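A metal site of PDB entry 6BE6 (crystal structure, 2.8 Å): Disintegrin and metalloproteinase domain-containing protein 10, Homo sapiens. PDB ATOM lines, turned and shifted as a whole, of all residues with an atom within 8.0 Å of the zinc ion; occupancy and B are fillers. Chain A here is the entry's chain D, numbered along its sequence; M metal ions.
The backbone carbonyl oxygen (O) of Ile 203 sits at hydrogen-bond distance from a ring nitrogen (ND1) of His 170 (2.9 Å). The side-chain carboxylate (OD1) of Asp 438 is in hydrogen-bond range of a ring nitrogen (ND1) of His 180 (2.6 Å). A ring nitrogen (ND1) of His 174 sits at hydrogen-bond distance from the backbone carbonyl oxygen (O) of Ser 178.
Of the 20 residues printed, 3 come within 4 Å of the zinc ion.
The zinc ion is bound by NE2 of His 174 (2.1 Å), NE2 of His 170 (2.1 Å) and NE2 of His 180 (2.3 Å).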
ATOM      1  N   GLY A 116     -20.373  14.615 -18.410  1.00  0.00           N
ATOM      2  CA  GLY A 116     -20.534  15.373 -17.189  1.00  0.00           C
ATOM      3  C   GLY A 116     -21.456  14.672 -16.223  1.00  0.00           C
ATOM      4  O   GLY A 116     -22.193  13.751 -16.584  1.00  0.00           O
ATOM      5  N   LEU A 117     -21.389  15.117 -14.964  1.00  0.00           N
ATOM      6  CA  LEU A 117     -22.217  14.590 -13.890  1.00  0.00           C
ATOM      7  C   LEU A 117     -22.687  15.730 -13.005  1.00  0.00           C
ATOM      8  O   LEU A 117     -21.921  16.654 -12.715  1.00  0.00           O
ATOM      9  CB  LEU A 117     -21.462  13.556 -13.036  1.00  0.00           C
ATOM     10  CG  LEU A 117     -21.750  12.076 -13.299  1.00  0.00           C
ATOM     11  CD1 LEU A 117     -21.025  11.214 -12.274  1.00  0.00           C
ATOM     12  CD2 LEU A 117     -23.240  11.810 -13.264  1.00  0.00           C
ATOM     13  N   ALA A 118     -23.947  15.657 -12.577  1.00  0.00           N
ATOM     14  CA  ALA A 118     -24.493  16.681 -11.694  1.00  0.00           C
ATOM     15  C   ALA A 118     -25.669  16.109 -10.911  1.00  0.00           C
ATOM     16  O   ALA A 118     -26.334  15.172 -11.369  1.00  0.00           O
ATOM     17  CB  ALA A 118     -24.938  17.927 -12.482  1.00  0.00           C
ATOM     18  N   VAL A 120     -29.419  16.279  -9.460  1.00  0.00           N
ATOM     19  CA  VAL A 120     -30.675  16.799  -9.980  1.00  0.00           C
ATOM     20  C   VAL A 120     -31.402  17.553  -8.863  1.00  0.00           C
ATOM     21  O   VAL A 120     -31.562  17.029  -7.765  1.00  0.00           O
ATOM     22  CB  VAL A 120     -31.558  15.673 -10.534  1.00  0.00           C
ATOM     23  CG1 VAL A 120     -32.919  16.201 -10.930  1.00  0.00           C
ATOM     24  CG2 VAL A 120     -30.878  15.007 -11.727  1.00  0.00           C
ATOM     25  N   THR A 167     -22.800  21.214 -22.785  1.00  0.00           N
ATOM     26  CA  THR A 167     -22.604  20.272 -21.683  1.00  0.00           C
ATOM     27  C   THR A 167     -22.655  20.984 -20.335  1.00  0.00           C
ATOM     28  O   THR A 167     -23.216  20.444 -19.370  1.00  0.00           O
ATOM     29  CB  THR A 167     -21.266  19.536 -21.856  1.00  0.00           C
ATOM     30  OG1 THR A 167     -21.228  18.918 -23.149  1.00  0.00           O
ATOM     31  CG2 THR A 167     -21.108  18.469 -20.787  1.00  0.00           C
ATOM     32  N   HIS A 170     -26.165  21.826 -19.649  1.00  0.00           N
ATOM     33  CA  HIS A 170     -26.901  20.575 -19.457  1.00  0.00           C
ATOM     34  C   HIS A 170     -26.767  20.084 -18.019  1.00  0.00           C
ATOM     35  O   HIS A 170     -27.756  19.648 -17.425  1.00  0.00           O
ATOM     36  CB  HIS A 170     -26.396  19.519 -20.440  1.00  0.00           C
ATOM     37  CG  HIS A 170     -27.037  18.179 -20.258  1.00  0.00           C
ATOM     38  ND1 HIS A 170     -28.199  17.809 -20.913  1.00  0.00           N
ATOM     39  CD2 HIS A 170     -26.687  17.113 -19.491  1.00  0.00           C
ATOM     40  CE1 HIS A 170     -28.528  16.582 -20.556  1.00  0.00           C
ATOM     41  NE2 HIS A 170     -27.626  16.140 -19.697  1.00  0.00           N
ATOM     42  N   GLU A 171     -25.569  20.143 -17.462  1.00  0.00           N
ATOM     43  CA  GLU A 171     -25.385  19.734 -16.065  1.00  0.00           C
ATOM     44  C   GLU A 171     -25.990  20.760 -15.117  1.00  0.00           C
ATOM     45  O   GLU A 171     -26.604  20.385 -14.105  1.00  0.00           O
ATOM     46  CB  GLU A 171     -23.900  19.525 -15.771  1.00  0.00           C
ATOM     47  CG  GLU A 171     -23.235  18.480 -16.665  1.00  0.00           C
ATOM     48  CD  GLU A 171     -23.933  17.126 -16.601  1.00  0.00           C
ATOM     49  OE1 GLU A 171     -24.340  16.713 -15.496  1.00  0.00           O
ATOM     50  OE2 GLU A 171     -24.077  16.493 -17.660  1.00  0.00           O
ATOM     51  N   GLY A 173     -28.492  22.484 -15.888  1.00  0.00           N
ATOM     52  CA  GLY A 173     -29.915  22.199 -16.008  1.00  0.00           C
ATOM     53  C   GLY A 173     -30.386  21.155 -15.015  1.00  0.00           C
ATOM     54  O   GLY A 173     -31.452  21.280 -14.416  1.00  0.00           O
ATOM     55  N   HIS A 174     -29.584  20.091 -14.823  1.00  0.00           N
ATOM     56  CA  HIS A 174     -29.881  19.129 -13.778  1.00  0.00           C
ATOM     57  C   HIS A 174     -29.886  19.789 -12.411  1.00  0.00           C
ATOM     58  O   HIS A 174     -30.771  19.526 -11.580  1.00  0.00           O
ATOM     59  CB  HIS A 174     -28.872  17.976 -13.812  1.00  0.00           C
ATOM     60  CG  HIS A 174     -29.048  17.052 -14.973  1.00  0.00           C
ATOM     61  ND1 HIS A 174     -30.248  16.456 -15.285  1.00  0.00           N
ATOM     62  CD2 HIS A 174     -28.152  16.592 -15.885  1.00  0.00           C
ATOM     63  CE1 HIS A 174     -30.101  15.687 -16.348  1.00  0.00           C
ATOM     64  NE2 HIS A 174     -28.839  15.757 -16.727  1.00  0.00           N
ATOM     65  N   SER A 178     -34.110  20.251 -13.810  1.00  0.00           N
ATOM     66  CA  SER A 178     -34.579  19.735 -15.084  1.00  0.00           C
ATOM     67  C   SER A 178     -34.106  18.298 -15.279  1.00  0.00           C
ATOM     68  O   SER A 178     -32.891  18.052 -15.267  1.00  0.00           O
ATOM     69  CB  SER A 178     -34.087  20.610 -16.233  1.00  0.00           C
ATOM     70  OG  SER A 178     -34.532  20.094 -17.478  1.00  0.00           O
ATOM     71  N   PRO A 179     -35.004  17.339 -15.446  1.00  0.00           N
ATOM     72  CA  PRO A 179     -34.579  15.978 -15.806  1.00  0.00           C
ATOM     73  C   PRO A 179     -34.377  15.839 -17.298  1.00  0.00           C
ATOM     74  O   PRO A 179     -34.408  16.835 -18.035  1.00  0.00           O
ATOM     75  CB  PRO A 179     -35.747  15.113 -15.306  1.00  0.00           C
ATOM     76  CG  PRO A 179     -36.938  15.995 -15.485  1.00  0.00           C
ATOM     77  CD  PRO A 179     -36.462  17.407 -15.213  1.00  0.00           C
ATOM     78  N   HIS A 180     -34.168  14.608 -17.769  1.00  0.00           N
ATOM     79  CA  HIS A 180     -34.002  14.385 -19.198  1.00  0.00           C
ATOM     80  C   HIS A 180     -35.343  14.493 -19.924  1.00  0.00           C
ATOM     81  O   HIS A 180     -36.398  14.146 -19.377  1.00  0.00           O
ATOM     82  CB  HIS A 180     -33.370  13.016 -19.458  1.00  0.00           C
ATOM     83  CG  HIS A 180     -31.911  12.965 -19.168  1.00  0.00           C
ATOM     84  ND1 HIS A 180     -31.328  11.954 -18.433  1.00  0.00           N
ATOM     85  CD2 HIS A 180     -30.897  13.795 -19.539  1.00  0.00           C
ATOM     86  CE1 HIS A 180     -30.018  12.173 -18.348  1.00  0.00           C
ATOM     87  NE2 HIS A 180     -29.735  13.278 -19.004  1.00  0.00           N
ATOM     88  N   ASP A 181     -35.297  14.996 -21.157  1.00  0.00           N
ATOM     89  CA  ASP A 181     -36.512  15.216 -21.917  1.00  0.00           C
ATOM     90  C   ASP A 181     -37.088  13.896 -22.409  1.00  0.00           C
ATOM     91  O   ASP A 181     -36.364  13.049 -22.945  1.00  0.00           O
ATOM     92  CB  ASP A 181     -36.228  16.143 -23.107  1.00  0.00           C
ATOM     93  CG  ASP A 181     -35.756  17.511 -22.685  1.00  0.00           C
ATOM     94  OD1 ASP A 181     -36.215  17.994 -21.630  1.00  0.00           O
ATOM     95  OD2 ASP A 181     -34.928  18.114 -23.405  1.00  0.00           O
ATOM     96  N   ILE A 203     -31.710  21.083 -25.169  1.00  0.00           N
ATOM     97  CA  ILE A 203     -30.432  21.040 -24.452  1.00  0.00           C
ATOM     98  C   ILE A 203     -30.414  19.945 -23.396  1.00  0.00           C
ATOM     99  O   ILE A 203     -29.354  19.354 -23.137  1.00  0.00           O
ATOM    100  CB  ILE A 203     -30.143  22.429 -23.854  1.00  0.00           C
ATOM    101  CG1 ILE A 203     -28.778  22.450 -23.167  1.00  0.00           C
ATOM    102  CG2 ILE A 203     -31.227  22.832 -22.874  1.00  0.00           C
ATOM    103  CD1 ILE A 203     -28.356  23.837 -22.778  1.00  0.00           C
ATOM    104  N   MET A 204     -31.560  19.630 -22.793  1.00  0.00           N
ATOM    105  CA  MET A 204     -31.645  18.559 -21.804  1.00  0.00           C
ATOM    106  C   MET A 204     -31.932  17.208 -22.438  1.00  0.00           C
ATOM    107  O   MET A 204     -32.476  16.317 -21.761  1.00  0.00           O
ATOM    108  CB  MET A 204     -32.718  18.891 -20.760  1.00  0.00           C
ATOM    109  CG  MET A 204     -32.392  20.105 -19.908  1.00  0.00           C
ATOM    110  SD  MET A 204     -30.817  19.939 -19.049  1.00  0.00           S
ATOM    111  CE  MET A 204     -31.107  18.447 -18.103  1.00  0.00           C
ATOM    112  N   TYR A 205     -31.589  17.029 -23.707  1.00  0.00           N
ATOM    113  CA  TYR A 205     -31.726  15.740 -24.364  1.00  0.00           C
ATOM    114  C   TYR A 205     -30.835  14.704 -23.683  1.00  0.00           C
ATOM    115  O   TYR A 205     -29.732  15.015 -23.227  1.00  0.00           O
ATOM    116  CB  TYR A 205     -31.365  15.876 -25.843  1.00  0.00           C
ATOM    117  CG  TYR A 205     -31.532  14.626 -26.673  1.00  0.00           C
ATOM    118  CD1 TYR A 205     -32.730  13.924 -26.689  1.00  0.00           C
ATOM    119  CD2 TYR A 205     -30.490  14.161 -27.456  1.00  0.00           C
ATOM    120  CE1 TYR A 205     -32.873  12.784 -27.460  1.00  0.00           C
ATOM    121  CE2 TYR A 205     -30.621  13.025 -28.234  1.00  0.00           C
ATOM    122  CZ  TYR A 205     -31.821  12.341 -28.224  1.00  0.00           C
ATOM    123  OH  TYR A 205     -31.961  11.209 -29.001  1.00  0.00           O
ATOM    124  N   ALA A 206     -31.328  13.468 -23.609  1.00  0.00           N
ATOM    125  CA  ALA A 206     -30.611  12.439 -22.855  1.00  0.00           C
ATOM    126  C   ALA A 206     -29.432  11.881 -23.635  1.00  0.00           C
ATOM    127  O   ALA A 206     -28.379  11.607 -23.060  1.00  0.00           O
ATOM    128  CB  ALA A 206     -31.568  11.325 -22.448  1.00  0.00           C
ATOM    129  N   ARG A 207     -29.588  11.691 -24.951  1.00  0.00           N
ATOM    130  CA  ARG A 207     -28.532  11.066 -25.737  1.00  0.00           C
ATOM    131  C   ARG A 207     -27.576  12.096 -26.334  1.00  0.00           C
ATOM    132  O   ARG A 207     -27.356  13.166 -25.750  1.00  0.00           O
ATOM    133  CB  ARG A 207     -29.142  10.202 -26.851  1.00  0.00           C
ATOM    134  CG  ARG A 207     -29.399   8.756 -26.429  1.00  0.00           C
ATOM    135  CD  ARG A 207     -30.648   8.636 -25.599  1.00  0.00           C
ATOM    136  NE  ARG A 207     -31.851   8.674 -26.432  1.00  0.00           N
ATOM    137  CZ  ARG A 207     -32.461   7.603 -26.910  1.00  0.00           C
ATOM    138  NH1 ARG A 207     -33.548   7.734 -27.666  1.00  0.00           N
ATOM    139  NH2 ARG A 207     -31.985   6.396 -26.640  1.00  0.00           N
ATOM    140  N   ALA A 437     -28.016   6.792 -20.221  1.00  0.00           N
ATOM    141  CA  ALA A 437     -27.738   7.649 -19.073  1.00  0.00           C
ATOM    142  C   ALA A 437     -28.792   7.538 -17.981  1.00  0.00           C
ATOM    143  O   ALA A 437     -28.495   7.818 -16.813  1.00  0.00           O
ATOM    144  CB  ALA A 437     -27.606   9.108 -19.514  1.00  0.00           C
ATOM    145  N   ASP A 438     -30.013   7.152 -18.330  1.00  0.00           N
ATOM    146  CA  ASP A 438     -31.081   6.969 -17.346  1.00  0.00           C
ATOM    147  C   ASP A 438     -31.043   5.526 -16.858  1.00  0.00           C
ATOM    148  O   ASP A 438     -31.501   4.617 -17.554  1.00  0.00           O
ATOM    149  CB  ASP A 438     -32.439   7.324 -17.963  1.00  0.00           C
ATOM    150  CG  ASP A 438     -32.532   8.796 -18.331  1.00  0.00           C
ATOM    151  OD1 ASP A 438     -32.142   9.642 -17.502  1.00  0.00           O
ATOM    152  OD2 ASP A 438     -32.993   9.096 -19.454  1.00  0.00           O
HETATM  153 ZN    ZN M   1     -28.045  14.641 -18.284  1.00  0.00          ZN
